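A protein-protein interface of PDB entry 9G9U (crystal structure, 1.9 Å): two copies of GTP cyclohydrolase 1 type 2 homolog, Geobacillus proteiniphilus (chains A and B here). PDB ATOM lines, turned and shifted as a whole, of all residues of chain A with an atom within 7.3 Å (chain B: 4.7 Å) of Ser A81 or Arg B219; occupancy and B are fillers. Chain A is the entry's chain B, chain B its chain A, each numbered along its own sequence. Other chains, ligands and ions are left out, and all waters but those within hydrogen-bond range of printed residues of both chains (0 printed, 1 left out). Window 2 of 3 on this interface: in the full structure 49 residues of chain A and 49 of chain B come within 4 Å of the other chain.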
ATOM      1  N   MET A  76       0.173   2.415 -16.881  1.00  0.00           N
ATOM      2  CA  MET A  76       0.398   3.355 -15.769  1.00  0.00           C
ATOM      3  C   MET A  76       1.875   3.695 -15.509  1.00  0.00           C
ATOM      4  O   MET A  76       2.163   4.456 -14.589  1.00  0.00           O
ATOM      5  CB  MET A  76      -0.293   2.943 -14.442  1.00  0.00           C
ATOM      6  CG  MET A  76       0.220   1.644 -13.775  1.00  0.00           C
ATOM      7  SD  MET A  76       0.194   1.447 -11.961  1.00  0.00           S
ATOM      8  CE  MET A  76       0.182  -0.345 -11.749  1.00  0.00           C
ATOM      9  N   MET A  77       2.805   3.165 -16.291  1.00  0.00           N
ATOM     10  CA  MET A  77       4.135   3.755 -16.418  1.00  0.00           C
ATOM     11  C   MET A  77       4.126   4.958 -17.341  1.00  0.00           C
ATOM     12  O   MET A  77       4.909   5.898 -17.152  1.00  0.00           O
ATOM     13  CB  MET A  77       5.139   2.719 -16.958  1.00  0.00           C
ATOM     14  CG  MET A  77       6.621   3.065 -16.889  1.00  0.00           C
ATOM     15  SD  MET A  77       7.572   1.548 -17.164  1.00  0.00           S
ATOM     16  CE  MET A  77       8.695   2.047 -18.471  1.00  0.00           C
ATOM     17  N   GLN A  78       3.217   4.938 -18.313  1.00  0.00           N
ATOM     18  CA  GLN A  78       3.076   6.022 -19.274  1.00  0.00           C
ATOM     19  C   GLN A  78       2.636   7.300 -18.579  1.00  0.00           C
ATOM     20  O   GLN A  78       3.374   8.295 -18.545  1.00  0.00           O
ATOM     21  CB  GLN A  78       2.078   5.596 -20.361  1.00  0.00           C
ATOM     22  CG  GLN A  78       2.472   4.299 -21.071  1.00  0.00           C
ATOM     23  CD  GLN A  78       3.981   4.181 -21.303  1.00  0.00           C
ATOM     24  OE1 GLN A  78       4.554   4.921 -22.109  1.00  0.00           O
ATOM     25  NE2 GLN A  78       4.627   3.254 -20.592  1.00  0.00           N
ATOM     26  N   LYS A  79       1.436   7.284 -18.004  1.00  0.00           N
ATOM     27  CA  LYS A  79       1.030   8.354 -17.112  1.00  0.00           C
ATOM     28  C   LYS A  79       1.651   8.148 -15.734  1.00  0.00           C
ATOM     29  O   LYS A  79       2.361   7.167 -15.468  1.00  0.00           O
ATOM     30  CB  LYS A  79      -0.490   8.438 -17.030  1.00  0.00           C
ATOM     31  CG  LYS A  79      -1.189   7.956 -18.287  1.00  0.00           C
ATOM     32  CD  LYS A  79      -2.684   7.758 -18.077  1.00  0.00           C
ATOM     33  CE  LYS A  79      -3.478   9.002 -18.479  1.00  0.00           C
ATOM     34  NZ  LYS A  79      -4.899   8.680 -18.828  1.00  0.00           N
ATOM     35  N   ASP A  80       1.352   9.106 -14.854  1.00  0.00           N
ATOM     36  CA  ASP A  80       1.965   9.278 -13.547  1.00  0.00           C
ATOM     37  C   ASP A  80       3.375   9.845 -13.665  1.00  0.00           C
ATOM     38  O   ASP A  80       4.286   9.187 -14.184  1.00  0.00           O
ATOM     39  CB  ASP A  80       1.976   7.963 -12.761  1.00  0.00           C
ATOM     40  CG  ASP A  80       2.154   8.203 -11.294  1.00  0.00           C
ATOM     41  OD1 ASP A  80       3.248   8.653 -10.904  1.00  0.00           O
ATOM     42  OD2 ASP A  80       1.194   7.981 -10.552  1.00  0.00           O
ATOM     43  N   SER A  81       3.544  11.067 -13.152  1.00  0.00           N
ATOM     44  CA  SER A  81       4.817  11.769 -13.245  1.00  0.00           C
ATOM     45  C   SER A  81       5.909  11.109 -12.409  1.00  0.00           C
ATOM     46  O   SER A  81       7.098  11.331 -12.662  1.00  0.00           O
ATOM     47  CB  SER A  81       4.624  13.220 -12.803  1.00  0.00           C
ATOM     48  OG  SER A  81       3.819  13.278 -11.637  1.00  0.00           O
ATOM     49  N   VAL A  82       5.530  10.310 -11.408  1.00  0.00           N
ATOM     50  CA  VAL A  82       6.514   9.647 -10.562  1.00  0.00           C
ATOM     51  C   VAL A  82       7.316   8.642 -11.374  1.00  0.00           C
ATOM     52  O   VAL A  82       8.553   8.664 -11.381  1.00  0.00           O
ATOM     53  CB  VAL A  82       5.812   8.973  -9.370  1.00  0.00           C
ATOM     54  CG1 VAL A  82       6.800   8.110  -8.602  1.00  0.00           C
ATOM     55  CG2 VAL A  82       5.144  10.028  -8.489  1.00  0.00           C
ATOM     56  N   TYR A  83       6.616   7.744 -12.077  1.00  0.00           N
ATOM     57  CA  TYR A  83       7.268   6.818 -12.996  1.00  0.00           C
ATOM     58  C   TYR A  83       8.119   7.557 -14.019  1.00  0.00           C
ATOM     59  O   TYR A  83       9.266   7.173 -14.275  1.00  0.00           O
ATOM     60  CB  TYR A  83       6.211   5.991 -13.719  1.00  0.00           C
ATOM     61  CG  TYR A  83       5.453   4.976 -12.891  1.00  0.00           C
ATOM     62  CD1 TYR A  83       4.491   5.371 -11.963  1.00  0.00           C
ATOM     63  CD2 TYR A  83       5.655   3.618 -13.081  1.00  0.00           C
ATOM     64  CE1 TYR A  83       3.771   4.430 -11.222  1.00  0.00           C
ATOM     65  CE2 TYR A  83       4.936   2.677 -12.357  1.00  0.00           C
ATOM     66  CZ  TYR A  83       4.001   3.085 -11.431  1.00  0.00           C
ATOM     67  OH  TYR A  83       3.305   2.135 -10.721  1.00  0.00           O
ATOM     68  N   GLN A  84       7.559   8.615 -14.618  1.00  0.00           N
ATOM     69  CA  GLN A  84       8.242   9.347 -15.682  1.00  0.00           C
ATOM     70  C   GLN A  84       9.570   9.917 -15.205  1.00  0.00           C
ATOM     71  O   GLN A  84      10.607   9.741 -15.860  1.00  0.00           O
ATOM     72  CB  GLN A  84       7.345  10.472 -16.204  1.00  0.00           C
ATOM     73  CG  GLN A  84       6.066  10.019 -16.893  1.00  0.00           C
ATOM     74  CD  GLN A  84       5.046  11.149 -17.031  1.00  0.00           C
ATOM     75  OE1 GLN A  84       5.392  12.334 -16.961  1.00  0.00           O
ATOM     76  NE2 GLN A  84       3.784  10.785 -17.226  1.00  0.00           N
ATOM     77  N   GLU A  85       9.552  10.619 -14.069  1.00  0.00           N
ATOM     78  CA  GLU A  85      10.767  11.262 -13.585  1.00  0.00           C
ATOM     79  C   GLU A  85      11.811  10.231 -13.176  1.00  0.00           C
ATOM     80  O   GLU A  85      13.015  10.472 -13.317  1.00  0.00           O
ATOM     81  CB  GLU A  85      10.442  12.211 -12.422  1.00  0.00           C
ATOM     82  CG  GLU A  85      11.671  12.803 -11.719  1.00  0.00           C
ATOM     83  CD  GLU A  85      12.412  13.832 -12.571  1.00  0.00           C
ATOM     84  OE1 GLU A  85      11.962  14.109 -13.705  1.00  0.00           O
ATOM     85  OE2 GLU A  85      13.447  14.361 -12.108  1.00  0.00           O
ATOM     86  N   LYS A  86      11.376   9.057 -12.699  1.00  0.00           N
ATOM     87  CA  LYS A  86      12.350   8.027 -12.357  1.00  0.00           C
ATOM     88  C   LYS A  86      13.016   7.463 -13.605  1.00  0.00           C
ATOM     89  O   LYS A  86      14.229   7.227 -13.607  1.00  0.00           O
ATOM     90  CB  LYS A  86      11.704   6.902 -11.548  1.00  0.00           C
ATOM     91  CG  LYS A  86      12.746   5.932 -10.972  1.00  0.00           C
ATOM     92  CD  LYS A  86      12.086   4.865 -10.113  1.00  0.00           C
ATOM     93  CE  LYS A  86      13.092   4.107  -9.253  1.00  0.00           C
ATOM     94  NZ  LYS A  86      12.399   3.266  -8.217  1.00  0.00           N
ATOM     95  N   ILE A  87      12.235   7.233 -14.668  1.00  0.00           N
ATOM     96  CA  ILE A  87      12.786   6.770 -15.942  1.00  0.00           C
ATOM     97  C   ILE A  87      13.771   7.783 -16.510  1.00  0.00           C
ATOM     98  O   ILE A  87      14.836   7.418 -17.022  1.00  0.00           O
ATOM     99  CB  ILE A  87      11.644   6.487 -16.932  1.00  0.00           C
ATOM    100  CG1 ILE A  87      10.862   5.262 -16.492  1.00  0.00           C
ATOM    101  CG2 ILE A  87      12.171   6.348 -18.359  1.00  0.00           C
ATOM    102  CD1 ILE A  87       9.463   5.246 -17.006  1.00  0.00           C
ATOM    103  N   ARG A  88      13.411   9.063 -16.443  1.00  0.00           N
ATOM    104  CA  ARG A  88      14.299  10.134 -16.876  1.00  0.00           C
ATOM    105  C   ARG A  88      15.619  10.098 -16.111  1.00  0.00           C
ATOM    106  O   ARG A  88      16.699  10.216 -16.705  1.00  0.00           O
ATOM    107  CB  ARG A  88      13.584  11.472 -16.688  1.00  0.00           C
ATOM    108  CG  ARG A  88      14.362  12.685 -17.150  1.00  0.00           C
ATOM    109  CD  ARG A  88      13.603  13.969 -16.887  1.00  0.00           C
ATOM    110  NE  ARG A  88      12.163  13.753 -17.012  1.00  0.00           N
ATOM    111  CZ  ARG A  88      11.498  13.702 -18.168  1.00  0.00           C
ATOM    112  NH1 ARG A  88      12.133  13.868 -19.324  1.00  0.00           N
ATOM    113  NH2 ARG A  88      10.186  13.483 -18.161  1.00  0.00           N
ATOM    114  N   GLU B 190      -3.099   9.900  -8.973  1.00  0.00           N
ATOM    115  CA  GLU B 190      -3.231  11.008  -9.911  1.00  0.00           C
ATOM    116  C   GLU B 190      -4.584  11.013 -10.616  1.00  0.00           C
ATOM    117  O   GLU B 190      -5.055  12.086 -11.001  1.00  0.00           O
ATOM    118  CB  GLU B 190      -2.063  10.979 -10.919  1.00  0.00           C
ATOM    119  CG  GLU B 190      -0.701  11.048 -10.196  1.00  0.00           C
ATOM    120  CD  GLU B 190       0.403  11.721 -11.001  1.00  0.00           C
ATOM    121  OE1 GLU B 190       1.528  11.863 -10.458  1.00  0.00           O
ATOM    122  OE2 GLU B 190       0.160  12.095 -12.166  1.00  0.00           O
ATOM    123  N   ALA B 214       7.786   9.273  -4.771  1.00  0.00           N
ATOM    124  CA  ALA B 214       7.055  10.517  -4.994  1.00  0.00           C
ATOM    125  C   ALA B 214       7.534  11.599  -4.035  1.00  0.00           C
ATOM    126  O   ALA B 214       7.778  12.743  -4.442  1.00  0.00           O
ATOM    127  CB  ALA B 214       5.544  10.283  -4.842  1.00  0.00           C
ATOM    128  N   VAL B 215       7.724  11.244  -2.768  1.00  0.00           N
ATOM    129  CA  VAL B 215       8.194  12.223  -1.801  1.00  0.00           C
ATOM    130  C   VAL B 215       9.635  12.623  -2.109  1.00  0.00           C
ATOM    131  O   VAL B 215      10.014  13.792  -1.961  1.00  0.00           O
ATOM    132  CB  VAL B 215       8.034  11.671  -0.374  1.00  0.00           C
ATOM    133  CG1 VAL B 215       8.719  12.585   0.619  1.00  0.00           C
ATOM    134  CG2 VAL B 215       6.537  11.535  -0.055  1.00  0.00           C
ATOM    135  N   GLN B 217      10.841  12.918  -5.006  1.00  0.00           N
ATOM    136  CA  GLN B 217      10.715  13.819  -6.139  1.00  0.00           C
ATOM    137  C   GLN B 217      10.040  15.136  -5.771  1.00  0.00           C
ATOM    138  O   GLN B 217       9.766  15.944  -6.662  1.00  0.00           O
ATOM    139  CB  GLN B 217       9.929  13.128  -7.264  1.00  0.00           C
ATOM    140  CG  GLN B 217      10.616  11.894  -7.838  1.00  0.00           C
ATOM    141  CD  GLN B 217       9.744  11.146  -8.826  1.00  0.00           C
ATOM    142  OE1 GLN B 217       8.646  11.597  -9.166  1.00  0.00           O
ATOM    143  NE2 GLN B 217      10.219  10.003  -9.287  1.00  0.00           N
ATOM    144  N   GLY B 218       9.748  15.370  -4.493  1.00  0.00           N
ATOM    145  CA  GLY B 218       9.161  16.617  -4.063  1.00  0.00           C
ATOM    146  C   GLY B 218       7.662  16.623  -3.868  1.00  0.00           C
ATOM    147  O   GLY B 218       7.116  17.656  -3.433  1.00  0.00           O
ATOM    148  N   ARG B 219       6.962  15.531  -4.165  1.00  0.00           N
ATOM    149  CA  ARG B 219       5.520  15.562  -3.970  1.00  0.00           C
ATOM    150  C   ARG B 219       5.194  15.415  -2.490  1.00  0.00           C
ATOM    151  O   ARG B 219       5.898  14.730  -1.732  1.00  0.00           O
ATOM    152  CB  ARG B 219       4.827  14.460  -4.769  1.00  0.00           C
ATOM    153  CG  ARG B 219       5.470  14.186  -6.108  1.00  0.00           C
ATOM    154  CD  ARG B 219       4.936  15.066  -7.218  1.00  0.00           C
ATOM    155  NE  ARG B 219       5.179  14.448  -8.523  1.00  0.00           N
ATOM    156  CZ  ARG B 219       6.377  14.360  -9.101  1.00  0.00           C
ATOM    157  NH1 ARG B 219       7.447  14.868  -8.505  1.00  0.00           N
ATOM    158  NH2 ARG B 219       6.505  13.780 -10.287  1.00  0.00           N
ATOM    159  N   GLN B 220       4.143  16.106  -2.070  1.00  0.00           N
ATOM    160  CA  GLN B 220       3.710  16.081  -0.682  1.00  0.00           C
ATOM    161  C   GLN B 220       2.567  15.078  -0.600  1.00  0.00           C
ATOM    162  O   GLN B 220       1.387  15.420  -0.698  1.00  0.00           O
ATOM    163  CB  GLN B 220       3.286  17.473  -0.231  1.00  0.00           C
ATOM    164  CG  GLN B 220       4.352  18.555  -0.368  1.00  0.00           C
ATOM    165  CD  GLN B 220       3.779  19.933  -0.090  1.00  0.00           C
ATOM    166  OE1 GLN B 220       2.945  20.435  -0.850  1.00  0.00           O
ATOM    167  NE2 GLN B 220       4.188  20.532   1.023  1.00  0.00           N
ATOM    168  N   LYS B 221       2.939  13.797  -0.481  1.00  0.00           N
ATOM    169  CA  LYS B 221       1.971  12.706  -0.451  1.00  0.00           C
ATOM    170  C   LYS B 221       2.300  11.779   0.705  1.00  0.00           C
ATOM    171  O   LYS B 221       3.428  11.753   1.212  1.00  0.00           O
ATOM    172  CB  LYS B 221       1.959  11.890  -1.763  1.00  0.00           C
ATOM    173  CG  LYS B 221       1.857  12.717  -3.033  1.00  0.00           C
ATOM    174  CD  LYS B 221       0.438  12.740  -3.578  1.00  0.00           C
ATOM    175  CE  LYS B 221       0.340  13.664  -4.820  1.00  0.00           C
ATOM    176  NZ  LYS B 221      -0.942  13.437  -5.566  1.00  0.00           N
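The side-chain hydroxyl (OG) of Ser A81 is in hydrogen-bond range of the side-chain carboxylate (OE1) of Glu B190 (2.9 Å).
The side-chain hydroxyl of Ser A81 sits at hydrogen-bond distance from the guanidinium group of Arg B219, 3.0 Å away.
The side-chain amide nitrogen (NE2) of Gln B217 sits at hydrogen-bond distance from the backbone carbonyl oxygen (O) of Val A82 (3.0 Å).
Of the printed residues of chain B, Asp A80 touches Glu B190.
Of chain B, only Glu B190, Gln B217 and Arg B219 come within 4 Å of Ser A81.
Of the printed residues of chain B, Val A82 touches Ala B214 (3.7 Å), Gln B217 (3.0 Å) and Arg B219 (3.8 Å).
Of the printed residues of chain B, Glu A85 touches Gln B217.
Of the printed residues of chain A, Ala B214 touches Val A82.
Of the printed residues of chain A, Gln B217 touches Ser A81, Val A82, Glu A85 and Lys A86.
Of chain A, only Ser A81 (3.0 Å) and Val A82 (3.8 Å) come within 4 Å of Arg B219.
Of the 8 printed residues of chain B, 4 touch a printed residue of chain A.
Printed residues of chain A that touch a printed residue of chain B: Asp A80, Ser A81, Val A82, Glu A85 and Lys A86.
Hydrophobic or aromatic side chains of chain A that line the printed part of chain B: Val A82.
Among the printed residues, 9 pairs touch across the chains.
Among the printed residues, no Asp or Glu carboxylate lies within 4 Å of a Lys or Arg side-chain nitrogen of the other chain.
No position is printed for both chains.
Of the 9 pairs that touch across the chains among the printed residues, none has its exchanged pair printed and touching as well.
The backbone carbonyl oxygen (O) of Gln B217 lies within hydrogen-bond range of the guanidinium group (NH1) of Arg B219, at 3.2 Å.
N of Arg B219 sits at hydrogen-bond distance from O of Ala B214 (2.9 Å).
OD1 of Asp A80 is in hydrogen-bond range of N of Val A82 (2.9 Å).
The side-chain carboxylate (OE1) of Glu A85 is in salt-bridge range of the guanidinium group (NE) of Arg A88.
The side-chain amide nitrogen (NE2) of Gln A84 lies close to the backbone carbonyl oxygen (O) of Asp A80 (3.5 Å).
CA of Asp A80 touches OE2 of Glu B190, at 3.6 Å.
Gln B217 touches Ser A81 (OE1 to O, 3.8 Å).
CG2 of Val A82 touches CB of Ala B214 (3.7 Å).
Arg B219 touches Val A82.
OE1 of Gln B217 touches CB of Glu A85 (3.8 Å).
Lys A86 touches Gln B217.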
